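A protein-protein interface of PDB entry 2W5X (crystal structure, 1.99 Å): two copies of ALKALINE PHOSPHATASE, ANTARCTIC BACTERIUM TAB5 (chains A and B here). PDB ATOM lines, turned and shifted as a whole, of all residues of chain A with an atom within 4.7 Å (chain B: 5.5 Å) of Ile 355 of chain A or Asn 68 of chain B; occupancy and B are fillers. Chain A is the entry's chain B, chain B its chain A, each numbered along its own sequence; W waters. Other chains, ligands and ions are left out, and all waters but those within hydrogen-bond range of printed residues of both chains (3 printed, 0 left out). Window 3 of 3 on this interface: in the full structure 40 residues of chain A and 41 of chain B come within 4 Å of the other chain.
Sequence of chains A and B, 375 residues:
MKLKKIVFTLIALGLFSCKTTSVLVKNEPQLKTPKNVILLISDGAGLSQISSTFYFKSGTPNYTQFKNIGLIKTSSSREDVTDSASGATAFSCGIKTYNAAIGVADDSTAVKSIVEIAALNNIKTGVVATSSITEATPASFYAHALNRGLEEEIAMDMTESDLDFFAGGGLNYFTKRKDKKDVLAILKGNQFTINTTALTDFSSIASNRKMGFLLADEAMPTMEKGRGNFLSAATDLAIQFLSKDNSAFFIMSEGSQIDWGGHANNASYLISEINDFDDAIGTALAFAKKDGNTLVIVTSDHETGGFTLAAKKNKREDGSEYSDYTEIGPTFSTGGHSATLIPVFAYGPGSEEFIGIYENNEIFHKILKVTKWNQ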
ATOM      1  N   ASN A  68      25.072  12.677 -23.829  1.00  0.00           N
ATOM      2  CA  ASN A  68      24.124  12.688 -22.733  1.00  0.00           C
ATOM      3  C   ASN A  68      24.653  11.938 -21.528  1.00  0.00           C
ATOM      4  O   ASN A  68      24.885  10.732 -21.591  1.00  0.00           O
ATOM      5  CB  ASN A  68      22.795  12.098 -23.190  1.00  0.00           C
ATOM      6  CG  ASN A  68      22.130  12.946 -24.256  1.00  0.00           C
ATOM      7  OD1 ASN A  68      22.176  14.173 -24.194  1.00  0.00           O
ATOM      8  ND2 ASN A  68      21.514  12.299 -25.235  1.00  0.00           N
ATOM      9  N   ILE A  69      24.831  12.666 -20.432  1.00  0.00           N
ATOM     10  CA  ILE A  69      25.433  12.127 -19.220  1.00  0.00           C
ATOM     11  C   ILE A  69      24.588  12.487 -17.998  1.00  0.00           C
ATOM     12  O   ILE A  69      24.071  13.603 -17.905  1.00  0.00           O
ATOM     13  CB  ILE A  69      26.865  12.689 -19.051  1.00  0.00           C
ATOM     14  CG1 ILE A  69      27.744  12.194 -20.207  1.00  0.00           C
ATOM     15  CG2 ILE A  69      27.437  12.309 -17.689  1.00  0.00           C
ATOM     16  CD1 ILE A  69      29.093  12.889 -20.315  1.00  0.00           C
ATOM     17  N   GLY A  70      24.421  11.526 -17.087  1.00  0.00           N
ATOM     18  CA  GLY A  70      23.688  11.733 -15.848  1.00  0.00           C
ATOM     19  C   GLY A  70      24.466  11.175 -14.666  1.00  0.00           C
ATOM     20  O   GLY A  70      25.584  10.687 -14.829  1.00  0.00           O
ATOM     21  N   SER A 351      17.884   8.768 -25.235  1.00  0.00           N
ATOM     22  CA  SER A 351      19.022   8.943 -24.326  1.00  0.00           C
ATOM     23  C   SER A 351      18.933  10.205 -23.466  1.00  0.00           C
ATOM     24  O   SER A 351      19.532  10.264 -22.394  1.00  0.00           O
ATOM     25  CB  SER A 351      20.351   8.922 -25.087  1.00  0.00           C
ATOM     26  OG  SER A 351      20.419   9.997 -26.009  1.00  0.00           O
ATOM     27  N   GLU A 352      18.188  11.210 -23.925  1.00  0.00           N
ATOM     28  CA  GLU A 352      18.050  12.463 -23.175  1.00  0.00           C
ATOM     29  C   GLU A 352      17.393  12.247 -21.810  1.00  0.00           C
ATOM     30  O   GLU A 352      17.610  13.016 -20.869  1.00  0.00           O
ATOM     31  CB  GLU A 352      17.255  13.510 -23.977  1.00  0.00           C
ATOM     32  CG  GLU A 352      17.949  14.028 -25.240  1.00  0.00           C
ATOM     33  CD  GLU A 352      17.839  13.082 -26.440  1.00  0.00           C
ATOM     34  OE1 GLU A 352      17.143  12.040 -26.360  1.00  0.00           O
ATOM     35  OE2 GLU A 352      18.457  13.391 -27.481  1.00  0.00           O
ATOM     36  N   GLU A 353      16.584  11.201 -21.701  1.00  0.00           N
ATOM     37  CA  GLU A 353      15.895  10.911 -20.448  1.00  0.00           C
ATOM     38  C   GLU A 353      16.870  10.601 -19.307  1.00  0.00           C
ATOM     39  O   GLU A 353      16.499  10.671 -18.134  1.00  0.00           O
ATOM     40  CB  GLU A 353      14.918   9.738 -20.625  1.00  0.00           C
ATOM     41  CG  GLU A 353      14.130   9.385 -19.365  1.00  0.00           C
ATOM     42  CD  GLU A 353      13.202  10.513 -18.916  1.00  0.00           C
ATOM     43  OE1 GLU A 353      12.699  11.251 -19.788  1.00  0.00           O
ATOM     44  OE2 GLU A 353      12.979  10.658 -17.691  1.00  0.00           O
ATOM     45  N   PHE A 354      18.113  10.269 -19.645  1.00  0.00           N
ATOM     46  CA  PHE A 354      19.052   9.769 -18.637  1.00  0.00           C
ATOM     47  C   PHE A 354      20.002  10.806 -18.050  1.00  0.00           C
ATOM     48  O   PHE A 354      20.893  10.455 -17.274  1.00  0.00           O
ATOM     49  CB  PHE A 354      19.823   8.552 -19.172  1.00  0.00           C
ATOM     50  CG  PHE A 354      18.951   7.351 -19.392  1.00  0.00           C
ATOM     51  CD1 PHE A 354      18.197   7.232 -20.553  1.00  0.00           C
ATOM     52  CD2 PHE A 354      18.839   6.367 -18.420  1.00  0.00           C
ATOM     53  CE1 PHE A 354      17.377   6.144 -20.759  1.00  0.00           C
ATOM     54  CE2 PHE A 354      18.018   5.275 -18.620  1.00  0.00           C
ATOM     55  CZ  PHE A 354      17.283   5.163 -19.791  1.00  0.00           C
ATOM     56  N   ILE A 355      19.804  12.077 -18.397  1.00  0.00           N
ATOM     57  CA  ILE A 355      20.687  13.138 -17.911  1.00  0.00           C
ATOM     58  C   ILE A 355      20.235  13.600 -16.525  1.00  0.00           C
ATOM     59  O   ILE A 355      19.291  13.047 -15.978  1.00  0.00           O
ATOM     60  CB  ILE A 355      20.760  14.331 -18.903  1.00  0.00           C
ATOM     61  CG1 ILE A 355      19.425  15.083 -18.966  1.00  0.00           C
ATOM     62  CG2 ILE A 355      21.162  13.847 -20.295  1.00  0.00           C
ATOM     63  CD1 ILE A 355      19.413  16.220 -20.000  1.00  0.00           C
ATOM     64  N   GLY A 356      20.900  14.604 -15.958  1.00  0.00           N
ATOM     65  CA  GLY A 356      20.568  15.054 -14.609  1.00  0.00           C
ATOM     66  C   GLY A 356      20.942  14.057 -13.516  1.00  0.00           C
ATOM     67  O   GLY A 356      21.704  13.114 -13.756  1.00  0.00           O
ATOM     68  N   ILE A 357      20.403  14.254 -12.312  1.00  0.00           N
ATOM     69  CA  ILE A 357      20.797  13.450 -11.148  1.00  0.00           C
ATOM     70  C   ILE A 357      19.609  12.736 -10.513  1.00  0.00           C
ATOM     71  O   ILE A 357      18.594  13.367 -10.206  1.00  0.00           O
ATOM     72  CB  ILE A 357      21.491  14.326 -10.082  1.00  0.00           C
ATOM     73  CG1 ILE A 357      22.677  15.084 -10.709  1.00  0.00           C
ATOM     74  CG2 ILE A 357      21.938  13.490  -8.887  1.00  0.00           C
ATOM     75  CD1 ILE A 357      23.449  15.965  -9.713  1.00  0.00           C
ATOM     76  N   TYR A 358      19.739  11.427 -10.295  1.00  0.00           N
ATOM     77  CA  TYR A 358      18.602  10.624  -9.821  1.00  0.00           C
ATOM     78  C   TYR A 358      19.033   9.352  -9.076  1.00  0.00           C
ATOM     79  O   TYR A 358      20.222   9.010  -9.035  1.00  0.00           O
ATOM     80  CB  TYR A 358      17.662  10.275 -10.993  1.00  0.00           C
ATOM     81  CG  TYR A 358      18.379   9.775 -12.231  1.00  0.00           C
ATOM     82  CD1 TYR A 358      18.596   8.416 -12.430  1.00  0.00           C
ATOM     83  CD2 TYR A 358      18.857  10.668 -13.197  1.00  0.00           C
ATOM     84  CE1 TYR A 358      19.269   7.950 -13.560  1.00  0.00           C
ATOM     85  CE2 TYR A 358      19.524  10.209 -14.328  1.00  0.00           C
ATOM     86  CZ  TYR A 358      19.730   8.848 -14.503  1.00  0.00           C
ATOM     87  OH  TYR A 358      20.398   8.377 -15.622  1.00  0.00           O
ATOM     88  N   PHE B  66      20.594  20.659 -11.782  1.00  0.00           N
ATOM     89  CA  PHE B  66      21.215  20.589 -13.099  1.00  0.00           C
ATOM     90  C   PHE B  66      20.734  19.385 -13.906  1.00  0.00           C
ATOM     91  O   PHE B  66      20.585  18.281 -13.376  1.00  0.00           O
ATOM     92  CB  PHE B  66      22.739  20.542 -12.974  1.00  0.00           C
ATOM     93  CG  PHE B  66      23.350  21.826 -12.480  1.00  0.00           C
ATOM     94  CD1 PHE B  66      23.772  21.949 -11.165  1.00  0.00           C
ATOM     95  CD2 PHE B  66      23.496  22.914 -13.332  1.00  0.00           C
ATOM     96  CE1 PHE B  66      24.338  23.130 -10.710  1.00  0.00           C
ATOM     97  CE2 PHE B  66      24.059  24.104 -12.887  1.00  0.00           C
ATOM     98  CZ  PHE B  66      24.480  24.218 -11.576  1.00  0.00           C
ATOM     99  N   LYS B  67      20.497  19.603 -15.196  1.00  0.00           N
ATOM    100  CA  LYS B  67      20.211  18.509 -16.117  1.00  0.00           C
ATOM    101  C   LYS B  67      21.399  18.274 -17.050  1.00  0.00           C
ATOM    102  O   LYS B  67      21.855  17.139 -17.228  1.00  0.00           O
ATOM    103  CB  LYS B  67      18.942  18.798 -16.930  1.00  0.00           C
ATOM    104  CG  LYS B  67      17.679  18.942 -16.085  1.00  0.00           C
ATOM    105  CD  LYS B  67      17.445  17.704 -15.228  1.00  0.00           C
ATOM    106  CE  LYS B  67      16.347  17.927 -14.178  1.00  0.00           C
ATOM    107  NZ  LYS B  67      16.292  16.827 -13.147  1.00  0.00           N
ATOM    108  N   ASN B  68      21.900  19.351 -17.650  1.00  0.00           N
ATOM    109  CA  ASN B  68      23.034  19.236 -18.554  1.00  0.00           C
ATOM    110  C   ASN B  68      24.339  19.063 -17.801  1.00  0.00           C
ATOM    111  O   ASN B  68      24.696  19.880 -16.951  1.00  0.00           O
ATOM    112  CB  ASN B  68      23.086  20.433 -19.498  1.00  0.00           C
ATOM    113  CG  ASN B  68      21.824  20.553 -20.318  1.00  0.00           C
ATOM    114  OD1 ASN B  68      21.331  19.557 -20.831  1.00  0.00           O
ATOM    115  ND2 ASN B  68      21.281  21.760 -20.422  1.00  0.00           N
ATOM    116  N   ILE B  69      25.034  17.974 -18.107  1.00  0.00           N
ATOM    117  CA  ILE B  69      26.230  17.583 -17.375  1.00  0.00           C
ATOM    118  C   ILE B  69      27.268  17.105 -18.373  1.00  0.00           C
ATOM    119  O   ILE B  69      26.941  16.389 -19.326  1.00  0.00           O
ATOM    120  CB  ILE B  69      25.920  16.435 -16.379  1.00  0.00           C
ATOM    121  CG1 ILE B  69      24.974  16.920 -15.280  1.00  0.00           C
ATOM    122  CG2 ILE B  69      27.204  15.883 -15.772  1.00  0.00           C
ATOM    123  CD1 ILE B  69      24.453  15.798 -14.382  1.00  0.00           C
ATOM    124  N   GLY B  70      28.513  17.508 -18.169  1.00  0.00           N
ATOM    125  CA  GLY B  70      29.593  17.060 -19.026  1.00  0.00           C
ATOM    126  C   GLY B  70      30.775  16.685 -18.167  1.00  0.00           C
ATOM    127  O   GLY B  70      30.675  16.710 -16.943  1.00  0.00           O
ATOM    128  N   VAL B 344      31.117  18.748 -15.082  1.00  0.00           N
ATOM    129  CA  VAL B 344      30.696  20.097 -15.416  1.00  0.00           C
ATOM    130  C   VAL B 344      29.170  20.143 -15.372  1.00  0.00           C
ATOM    131  O   VAL B 344      28.510  19.292 -15.962  1.00  0.00           O
ATOM    132  CB  VAL B 344      31.125  20.474 -16.837  1.00  0.00           C
ATOM    133  CG1 VAL B 344      30.577  21.836 -17.204  1.00  0.00           C
ATOM    134  CG2 VAL B 344      32.648  20.461 -16.953  1.00  0.00           C
ATOM    135  N   PHE B 345      28.606  21.123 -14.670  1.00  0.00           N
ATOM    136  CA  PHE B 345      27.157  21.280 -14.616  1.00  0.00           C
ATOM    137  C   PHE B 345      26.800  22.608 -15.264  1.00  0.00           C
ATOM    138  O   PHE B 345      27.469  23.607 -15.018  1.00  0.00           O
ATOM    139  CB  PHE B 345      26.658  21.243 -13.163  1.00  0.00           C
ATOM    140  CG  PHE B 345      27.130  20.037 -12.383  1.00  0.00           C
ATOM    141  CD1 PHE B 345      26.317  18.922 -12.243  1.00  0.00           C
ATOM    142  CD2 PHE B 345      28.382  20.029 -11.776  1.00  0.00           C
ATOM    143  CE1 PHE B 345      26.750  17.811 -11.523  1.00  0.00           C
ATOM    144  CE2 PHE B 345      28.824  18.920 -11.065  1.00  0.00           C
ATOM    145  CZ  PHE B 345      28.007  17.812 -10.935  1.00  0.00           C
ATOM    146  N   ALA B 346      25.762  22.630 -16.102  1.00  0.00           N
ATOM    147  CA  ALA B 346      25.374  23.890 -16.733  1.00  0.00           C
ATOM    148  C   ALA B 346      23.865  24.060 -16.761  1.00  0.00           C
ATOM    149  O   ALA B 346      23.125  23.126 -17.066  1.00  0.00           O
ATOM    150  CB  ALA B 346      25.959  24.011 -18.142  1.00  0.00           C
ATOM    151  N   SER B 351      23.309  26.040 -22.229  1.00  0.00           N
ATOM    152  CA  SER B 351      23.835  25.014 -21.317  1.00  0.00           C
ATOM    153  C   SER B 351      24.115  23.677 -22.023  1.00  0.00           C
ATOM    154  O   SER B 351      24.988  22.920 -21.592  1.00  0.00           O
ATOM    155  CB  SER B 351      22.892  24.800 -20.131  1.00  0.00           C
ATOM    156  OG  SER B 351      21.623  24.368 -20.590  1.00  0.00           O
ATOM    157  N   GLU B 352      23.391  23.396 -23.109  1.00  0.00           N
ATOM    158  CA  GLU B 352      23.609  22.158 -23.878  1.00  0.00           C
ATOM    159  C   GLU B 352      25.009  22.070 -24.488  1.00  0.00           C
ATOM    160  O   GLU B 352      25.470  20.993 -24.839  1.00  0.00           O
ATOM    161  CB  GLU B 352      22.577  22.005 -25.003  1.00  0.00           C
ATOM    162  CG  GLU B 352      21.175  21.661 -24.539  1.00  0.00           C
ATOM    163  CD  GLU B 352      20.352  22.893 -24.210  1.00  0.00           C
ATOM    164  OE1 GLU B 352      20.883  24.029 -24.350  1.00  0.00           O
ATOM    165  OE2 GLU B 352      19.173  22.720 -23.815  1.00  0.00           O
ATOM    166  N   ILE B 355      27.786  19.652 -22.425  1.00  0.00           N
ATOM    167  CA  ILE B 355      27.667  18.207 -22.190  1.00  0.00           C
ATOM    168  C   ILE B 355      28.771  17.445 -22.926  1.00  0.00           C
ATOM    169  O   ILE B 355      29.615  18.043 -23.592  1.00  0.00           O
ATOM    170  CB  ILE B 355      26.277  17.667 -22.625  1.00  0.00           C
ATOM    171  CG1 ILE B 355      26.134  17.694 -24.145  1.00  0.00           C
ATOM    172  CG2 ILE B 355      25.158  18.478 -21.976  1.00  0.00           C
ATOM    173  CD1 ILE B 355      24.781  17.180 -24.647  1.00  0.00           C
HETATM  174  O   HOH W   1      18.846  16.715 -11.996  1.00  0.00           O
HETATM  175  O   HOH W   2      16.518  14.169 -12.560  1.00  0.00           O
HETATM  176  O   HOH W   3      24.429  15.578 -19.804  1.00  0.00           O
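O of Lys 67 of chain B is in hydrogen-bond range of N of Gly 356 of chain A, 3.0 Å away.
The backbone carbonyl oxygen (O) of Asn 68 of chain B is in hydrogen-bond range of the backbone NH (N) of Ala 346 of chain B.
ND2 of Asn 68 of chain B sits at hydrogen-bond distance from OG of Ser 351 of chain B, 2.6 Å away.
Among the printed residues, pairs that only touch across the chains: Ile 69 of chain A with Ile 69 of chain B (3.7 Å), Ile 355 of chain A with Lys 67 of chain B (3.4 Å), Ile 355 of chain A with Asn 68 of chain B (3.9 Å), Gly 356 of chain A with Phe 66 of chain B (3.5 Å) and Gly 356 of chain A with Ile 69 of chain B (3.9 Å).
Printed residues of chain B within 4 Å of Ile 69 of chain A: Ile 69.
Of chain B, only Lys 67 and Asn 68 come within 4 Å of Ile 355 of chain A.
Of the printed residues of chain B, Gly 356 of chain A touches Phe 66, Lys 67 and Ile 69.
Of the printed residues of chain A, Lys 67 of chain B touches Ile 355 (3.4 Å) and Gly 356 (3.0 Å).
Of chain A, only Ile 355 comes within 4 Å of Asn 68 of chain B.
Of the printed residues of chain A, Ile 69 of chain B touches Ile 69 and Gly 356.
The nearest residue of chain B that does not touch Ile 355 of chain A is Ile 69 of chain B (5.2 Å).
Hydrophobic or aromatic side chains of chain B within 4 Å of the printed part of chain A: Ile 69.
Among the printed residues, no Asp or Glu carboxylate lies within 4 Å of a Lys or Arg side-chain nitrogen of the other chain.
Ile 69 of chain A touches its own counterpart, Ile 69 of chain B.
Ile 355 of chain A touches Asn 68 of chain B, but with the chains exchanged Asn 68 of chain A does not touch Ile 355 of chain B (4.004 Å).
Positions printed for both chains: 68, 69, 70, 351, 352 and 355.
Of the 6 pairs that touch across the chains among the printed residues, 1 has its exchanged pair printed and touching as well.
Water W3 bridges the backbone carbonyl oxygen of Ile 69 of chain B (2.7 Å) and the backbone carbonyl oxygen of Ile 69 of chain A (2.8 Å).
Water W1 lies within hydrogen-bond range of O of Phe 66 of chain B, NZ of Lys 67 of chain B and N of Ile 357 of chain A.
Water W2 bridges the side-chain amino group of Lys 67 of chain B (2.7 Å) and the backbone carbonyl oxygen of Ile 357 of chain A (3.2 Å).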
